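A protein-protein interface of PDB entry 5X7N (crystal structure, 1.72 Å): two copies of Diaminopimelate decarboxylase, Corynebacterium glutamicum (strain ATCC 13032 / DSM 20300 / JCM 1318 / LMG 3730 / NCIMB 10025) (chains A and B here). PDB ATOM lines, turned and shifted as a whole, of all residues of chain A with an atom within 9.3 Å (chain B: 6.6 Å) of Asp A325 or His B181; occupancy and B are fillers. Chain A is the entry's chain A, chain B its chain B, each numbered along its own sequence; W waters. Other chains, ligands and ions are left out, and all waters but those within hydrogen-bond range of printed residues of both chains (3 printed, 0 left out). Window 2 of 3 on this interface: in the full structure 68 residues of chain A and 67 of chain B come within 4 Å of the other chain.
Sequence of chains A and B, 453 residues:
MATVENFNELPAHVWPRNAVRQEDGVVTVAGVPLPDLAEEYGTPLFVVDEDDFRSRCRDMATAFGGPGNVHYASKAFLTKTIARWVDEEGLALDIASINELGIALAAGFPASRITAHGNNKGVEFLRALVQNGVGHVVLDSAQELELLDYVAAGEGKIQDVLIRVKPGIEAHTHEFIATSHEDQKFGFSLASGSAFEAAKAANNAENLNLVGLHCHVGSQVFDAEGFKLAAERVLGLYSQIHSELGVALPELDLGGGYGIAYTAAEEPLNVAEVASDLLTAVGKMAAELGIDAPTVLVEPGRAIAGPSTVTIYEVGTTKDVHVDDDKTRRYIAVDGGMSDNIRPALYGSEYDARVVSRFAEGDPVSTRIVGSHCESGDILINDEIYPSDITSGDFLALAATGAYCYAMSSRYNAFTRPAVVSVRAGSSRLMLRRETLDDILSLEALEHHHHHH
The side-chain carboxylate of Asp A325 lies within hydrogen-bond range of a ring nitrogen (NE2) of His B181. The side-chain carboxylate (OD1) of Asp B183 is in hydrogen-bond range of the side-chain hydroxyl (OH) of Tyr A331, at 2.6 Å. NE2 of His B181 lies close to O of Asp A324.
Water W1 lies within hydrogen-bond range of the side-chain hydroxyl of Ser B189, the backbone carbonyl oxygen of His A322 and the side-chain amino group of Lys B166. Water W3 bridges OH of Tyr A331 (2.9 Å) and O of Asp B183 (3.0 Å). Water W2 lies within hydrogen-bond range of OG1 of Thr B179 (3.2 Å) and O of Val A323 (3.3 Å).
Of chain B, only His B181 comes within 4 Å of Asp A325. Of chain A, only His A322, Val A323, Asp A324 and Asp A325 come within 4 Å of His B181. No residue of chain A comes within 4 Å of Ser B180. Of the printed residues of chain B, Val A321 touches Lys B166 (3.6 Å) and Glu B182 (3.5 Å). Of the printed residues of chain B, Val A323 touches His B181 and Asp B183. Printed residues of chain B within 4 Å of Asp A324: His B181. Printed residues of chain A within 4 Å of Lys B166: Val A321. The nearest residue of chain A that does not touch His B181 is Asp A326 (5.8 Å).
No position is printed for both chains. Of the 8 pairs that touch across the chains among the printed residues, none has its exchanged pair printed and touching as well.
Val A321 touches Lys B166 (CG1 to NZ, 3.6 Å). Glu B182 touches Val A321 (O to CG1, 3.5 Å). O of His A322 touches CB of His B181, at 3.4 Å. Val A323 touches His B181 (O to CB, 3.7 Å). OD1 of Asp B183 touches CG2 of Val A323, at 3.6 Å.
A ring nitrogen (ND1) of His A322 is in hydrogen-bond range of the backbone carbonyl oxygen (O) of Asp A324, 2.9 Å away. OG1 of Thr B179 sits close to O of His B181 (3.1 Å). ND1 of His A322 is in hydrogen-bond range of O of Lys A327, at 3.3 Å. A ring nitrogen (ND1) of His A322 sits close to the backbone carbonyl oxygen of Asp A325 (3.4 Å). The side-chain amino group of Lys B166 lies within hydrogen-bond range of the backbone carbonyl oxygen of Glu B182 (2.9 Å). OD1 of Asp A324 lies within hydrogen-bond range of N of Lys A327.
Of the 10 printed residues of chain A, 6 touch a printed residue of chain B. Hydrophobic or aromatic side chains of chain A that line the printed part of chain B: Val A321, His A322, Val A323 and Tyr A331. Printed residues of chain B that touch a printed residue of chain A: Lys B166, His B181, Glu B182 and Asp B183. Hydrophobic or aromatic side chains of chain B within 4 Å of the printed part of chain A: His B181. Among the printed residues, 8 pairs touch across the chains. Among the printed residues, no Asp or Glu carboxylate lies within 4 Å of a Lys or Arg side-chain nitrogen of the other chain.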
ATOM      1  N   ASP A 320      12.312  15.663  20.788  1.00  0.00           N
ATOM      2  CA  ASP A 320      11.499  15.738  19.573  1.00  0.00           C
ATOM      3  C   ASP A 320      11.277  17.200  19.233  1.00  0.00           C
ATOM      4  O   ASP A 320      10.831  17.980  20.106  1.00  0.00           O
ATOM      5  CB  ASP A 320      10.155  15.061  19.812  1.00  0.00           C
ATOM      6  CG  ASP A 320      10.269  13.560  19.946  1.00  0.00           C
ATOM      7  OD1 ASP A 320      11.102  12.927  19.296  1.00  0.00           O
ATOM      8  OD2 ASP A 320       9.499  13.024  20.734  1.00  0.00           O
ATOM      9  N   VAL A 321      11.551  17.545  17.962  1.00  0.00           N
ATOM     10  CA  VAL A 321      11.374  18.891  17.414  1.00  0.00           C
ATOM     11  C   VAL A 321      10.375  18.894  16.291  1.00  0.00           C
ATOM     12  O   VAL A 321      10.583  18.200  15.289  1.00  0.00           O
ATOM     13  CB  VAL A 321      12.748  19.379  16.873  1.00  0.00           C
ATOM     14  CG1 VAL A 321      12.616  20.754  16.193  1.00  0.00           C
ATOM     15  CG2 VAL A 321      13.757  19.422  18.032  1.00  0.00           C
ATOM     16  N   HIS A 322       9.279  19.660  16.432  1.00  0.00           N
ATOM     17  CA  HIS A 322       8.351  19.787  15.281  1.00  0.00           C
ATOM     18  C   HIS A 322       9.025  20.667  14.217  1.00  0.00           C
ATOM     19  O   HIS A 322       9.626  21.705  14.526  1.00  0.00           O
ATOM     20  CB  HIS A 322       6.998  20.402  15.663  1.00  0.00           C
ATOM     21  CG  HIS A 322       5.925  19.404  15.858  1.00  0.00           C
ATOM     22  ND1 HIS A 322       5.216  18.863  14.804  1.00  0.00           N
ATOM     23  CD2 HIS A 322       5.433  18.825  16.984  1.00  0.00           C
ATOM     24  CE1 HIS A 322       4.354  17.969  15.271  1.00  0.00           C
ATOM     25  NE2 HIS A 322       4.461  17.931  16.587  1.00  0.00           N
ATOM     26  N   VAL A 323       8.981  20.214  12.988  1.00  0.00           N
ATOM     27  CA  VAL A 323       9.598  20.915  11.858  1.00  0.00           C
ATOM     28  C   VAL A 323       8.548  21.769  11.131  1.00  0.00           C
ATOM     29  O   VAL A 323       8.865  22.854  10.617  1.00  0.00           O
ATOM     30  CB  VAL A 323      10.257  19.906  10.945  1.00  0.00           C
ATOM     31  CG1 VAL A 323      10.852  20.586   9.729  1.00  0.00           C
ATOM     32  CG2 VAL A 323      11.365  19.232  11.751  1.00  0.00           C
ATOM     33  N   ASP A 324       7.321  21.271  11.133  1.00  0.00           N
ATOM     34  CA  ASP A 324       6.105  22.045  10.733  1.00  0.00           C
ATOM     35  C   ASP A 324       5.007  21.577  11.688  1.00  0.00           C
ATOM     36  O   ASP A 324       5.302  20.899  12.714  1.00  0.00           O
ATOM     37  CB  ASP A 324       5.741  21.854   9.240  1.00  0.00           C
ATOM     38  CG  ASP A 324       5.640  20.387   8.824  1.00  0.00           C
ATOM     39  OD1 ASP A 324       4.946  19.606   9.517  1.00  0.00           O
ATOM     40  OD2 ASP A 324       6.308  19.977   7.841  1.00  0.00           O
ATOM     41  N   ASP A 325       3.736  21.897  11.407  1.00  0.00           N
ATOM     42  CA  ASP A 325       2.632  21.418  12.292  1.00  0.00           C
ATOM     43  C   ASP A 325       2.545  19.865  12.359  1.00  0.00           C
ATOM     44  O   ASP A 325       2.113  19.325  13.374  1.00  0.00           O
ATOM     45  CB  ASP A 325       1.258  21.983  11.867  1.00  0.00           C
ATOM     46  CG  ASP A 325       1.154  23.515  12.035  1.00  0.00           C
ATOM     47  OD1 ASP A 325       1.705  24.043  13.051  1.00  0.00           O
ATOM     48  OD2 ASP A 325       0.497  24.160  11.161  1.00  0.00           O
ATOM     49  N   ASP A 326       2.961  19.165  11.289  1.00  0.00           N
ATOM     50  CA  ASP A 326       2.710  17.711  11.183  1.00  0.00           C
ATOM     51  C   ASP A 326       3.930  16.797  11.308  1.00  0.00           C
ATOM     52  O   ASP A 326       3.763  15.683  11.746  1.00  0.00           O
ATOM     53  CB  ASP A 326       1.892  17.398   9.920  1.00  0.00           C
ATOM     54  CG  ASP A 326       0.438  17.895  10.041  1.00  0.00           C
ATOM     55  OD1 ASP A 326      -0.250  17.464  11.004  1.00  0.00           O
ATOM     56  OD2 ASP A 326       0.003  18.734   9.204  1.00  0.00           O
ATOM     57  N   LYS A 327       5.131  17.252  10.955  1.00  0.00           N
ATOM     58  CA  LYS A 327       6.308  16.343  10.976  1.00  0.00           C
ATOM     59  C   LYS A 327       7.248  16.656  12.191  1.00  0.00           C
ATOM     60  O   LYS A 327       7.406  17.823  12.590  1.00  0.00           O
ATOM     61  CB  LYS A 327       7.098  16.384   9.658  1.00  0.00           C
ATOM     62  CG  LYS A 327       6.268  16.547   8.378  1.00  0.00           C
ATOM     63  CD  LYS A 327       5.159  15.518   8.128  1.00  0.00           C
ATOM     64  CE  LYS A 327       4.190  16.075   7.090  1.00  0.00           C
ATOM     65  NZ  LYS A 327       3.365  15.030   6.441  1.00  0.00           N
ATOM     66  N   THR A 328       7.793  15.591  12.770  1.00  0.00           N
ATOM     67  CA  THR A 328       8.698  15.658  13.912  1.00  0.00           C
ATOM     68  C   THR A 328      10.067  15.146  13.493  1.00  0.00           C
ATOM     69  O   THR A 328      10.168  14.195  12.751  1.00  0.00           O
ATOM     70  CB  THR A 328       8.112  14.810  15.008  1.00  0.00           C
ATOM     71  OG1 THR A 328       6.786  15.337  15.299  1.00  0.00           O
ATOM     72  CG2 THR A 328       9.012  14.848  16.255  1.00  0.00           C
ATOM     73  N   TYR A 331      15.993  14.671  17.639  1.00  0.00           N
ATOM     74  CA  TYR A 331      17.384  15.144  17.732  1.00  0.00           C
ATOM     75  C   TYR A 331      18.054  14.344  18.806  1.00  0.00           C
ATOM     76  O   TYR A 331      17.550  14.281  19.913  1.00  0.00           O
ATOM     77  CB  TYR A 331      17.456  16.645  18.086  1.00  0.00           C
ATOM     78  CG  TYR A 331      17.316  17.558  16.870  1.00  0.00           C
ATOM     79  CD1 TYR A 331      16.101  17.692  16.156  1.00  0.00           C
ATOM     80  CD2 TYR A 331      18.421  18.250  16.396  1.00  0.00           C
ATOM     81  CE1 TYR A 331      16.009  18.577  15.055  1.00  0.00           C
ATOM     82  CE2 TYR A 331      18.343  19.088  15.310  1.00  0.00           C
ATOM     83  CZ  TYR A 331      17.131  19.280  14.661  1.00  0.00           C
ATOM     84  OH  TYR A 331      17.075  20.108  13.597  1.00  0.00           O
ATOM     85  N   LYS B 166      13.064  29.157  21.314  1.00  0.00           N
ATOM     86  CA  LYS B 166      13.141  29.316  19.836  1.00  0.00           C
ATOM     87  C   LYS B 166      12.008  30.199  19.374  1.00  0.00           C
ATOM     88  O   LYS B 166      10.873  29.764  19.317  1.00  0.00           O
ATOM     89  CB  LYS B 166      13.101  27.967  19.132  1.00  0.00           C
ATOM     90  CG  LYS B 166      14.379  27.135  19.394  1.00  0.00           C
ATOM     91  CD  LYS B 166      14.263  25.810  18.681  1.00  0.00           C
ATOM     92  CE  LYS B 166      13.036  25.017  18.977  1.00  0.00           C
ATOM     93  NZ  LYS B 166      12.994  23.729  18.229  1.00  0.00           N
ATOM     94  N   GLY B 168      11.356  31.436  16.470  1.00  0.00           N
ATOM     95  CA  GLY B 168      11.038  31.297  15.003  1.00  0.00           C
ATOM     96  C   GLY B 168      11.551  32.481  14.241  1.00  0.00           C
ATOM     97  O   GLY B 168      10.905  32.895  13.269  1.00  0.00           O
ATOM     98  N   THR B 179       9.480  31.981  11.069  1.00  0.00           N
ATOM     99  CA  THR B 179       8.773  30.706  10.980  1.00  0.00           C
ATOM    100  C   THR B 179       8.001  30.386  12.254  1.00  0.00           C
ATOM    101  O   THR B 179       8.203  31.082  13.266  1.00  0.00           O
ATOM    102  CB  THR B 179       9.769  29.637  10.716  1.00  0.00           C
ATOM    103  OG1 THR B 179       9.015  28.424  10.585  1.00  0.00           O
ATOM    104  CG2 THR B 179      10.797  29.566  11.897  1.00  0.00           C
ATOM    105  N   SER B 180       7.083  29.398  12.200  1.00  0.00           N
ATOM    106  CA  SER B 180       6.354  28.963  13.400  1.00  0.00           C
ATOM    107  C   SER B 180       7.158  27.895  14.174  1.00  0.00           C
ATOM    108  O   SER B 180       6.953  27.742  15.359  1.00  0.00           O
ATOM    109  CB  SER B 180       4.959  28.375  13.124  1.00  0.00           C
ATOM    110  OG  SER B 180       5.109  27.331  12.212  1.00  0.00           O
ATOM    111  N   HIS B 181       8.069  27.229  13.489  1.00  0.00           N
ATOM    112  CA  HIS B 181       8.953  26.216  14.148  1.00  0.00           C
ATOM    113  C   HIS B 181      10.403  26.386  13.695  1.00  0.00           C
ATOM    114  O   HIS B 181      10.625  26.667  12.557  1.00  0.00           O
ATOM    115  CB  HIS B 181       8.545  24.791  13.761  1.00  0.00           C
ATOM    116  CG  HIS B 181       7.078  24.505  13.851  1.00  0.00           C
ATOM    117  ND1 HIS B 181       6.444  24.223  15.042  1.00  0.00           N
ATOM    118  CD2 HIS B 181       6.119  24.467  12.898  1.00  0.00           C
ATOM    119  CE1 HIS B 181       5.151  24.038  14.828  1.00  0.00           C
ATOM    120  NE2 HIS B 181       4.923  24.197  13.535  1.00  0.00           N
ATOM    121  N   GLU B 182      11.369  26.118  14.558  1.00  0.00           N
ATOM    122  CA  GLU B 182      12.784  26.162  14.162  1.00  0.00           C
ATOM    123  C   GLU B 182      13.309  24.749  14.264  1.00  0.00           C
ATOM    124  O   GLU B 182      13.263  24.127  15.378  1.00  0.00           O
ATOM    125  CB  GLU B 182      13.657  27.086  15.063  1.00  0.00           C
ATOM    126  CG  GLU B 182      13.314  28.547  14.999  1.00  0.00           C
ATOM    127  CD  GLU B 182      14.317  29.443  15.680  1.00  0.00           C
ATOM    128  OE1 GLU B 182      13.965  30.371  16.401  1.00  0.00           O
ATOM    129  OE2 GLU B 182      15.540  29.252  15.367  1.00  0.00           O
ATOM    130  N   ASP B 183      13.789  24.228  13.136  1.00  0.00           N
ATOM    131  CA  ASP B 183      14.314  22.871  13.049  1.00  0.00           C
ATOM    132  C   ASP B 183      15.797  22.902  13.411  1.00  0.00           C
ATOM    133  O   ASP B 183      16.707  22.918  12.550  1.00  0.00           O
ATOM    134  CB  ASP B 183      14.080  22.407  11.617  1.00  0.00           C
ATOM    135  CG  ASP B 183      14.511  20.998  11.330  1.00  0.00           C
ATOM    136  OD1 ASP B 183      14.806  20.215  12.249  1.00  0.00           O
ATOM    137  OD2 ASP B 183      14.545  20.685  10.132  1.00  0.00           O
ATOM    138  N   SER B 189      10.638  25.044  22.002  1.00  0.00           N
ATOM    139  CA  SER B 189       9.712  25.748  21.095  1.00  0.00           C
ATOM    140  C   SER B 189       8.767  26.653  21.840  1.00  0.00           C
ATOM    141  O   SER B 189       8.145  26.277  22.843  1.00  0.00           O
ATOM    142  CB  SER B 189       8.725  24.862  20.234  1.00  0.00           C
ATOM    143  OG  SER B 189       9.415  23.875  19.584  1.00  0.00           O
ATOM    144  N   ALA B 191       6.169  27.925  19.994  1.00  0.00           N
ATOM    145  CA  ALA B 191       4.897  27.743  19.381  1.00  0.00           C
ATOM    146  C   ALA B 191       4.101  26.595  19.972  1.00  0.00           C
ATOM    147  O   ALA B 191       2.901  26.659  19.956  1.00  0.00           O
ATOM    148  CB  ALA B 191       5.063  27.555  17.887  1.00  0.00           C
ATOM    149  N   SER B 192       4.732  25.559  20.479  1.00  0.00           N
ATOM    150  CA  SER B 192       3.997  24.447  21.013  1.00  0.00           C
ATOM    151  C   SER B 192       3.578  24.633  22.417  1.00  0.00           C
ATOM    152  O   SER B 192       2.874  23.759  22.928  1.00  0.00           O
ATOM    153  CB  SER B 192       4.839  23.148  20.966  1.00  0.00           C
ATOM    154  OG  SER B 192       5.901  23.195  21.914  1.00  0.00           O
HETATM  155  O   HOH W   1      10.044  22.872  17.044  1.00  0.00           O
HETATM  156  O   HOH W   2       8.895  25.704   8.990  1.00  0.00           O
HETATM  157  O   HOH W   3      19.347  21.576  12.437  1.00  0.00           O
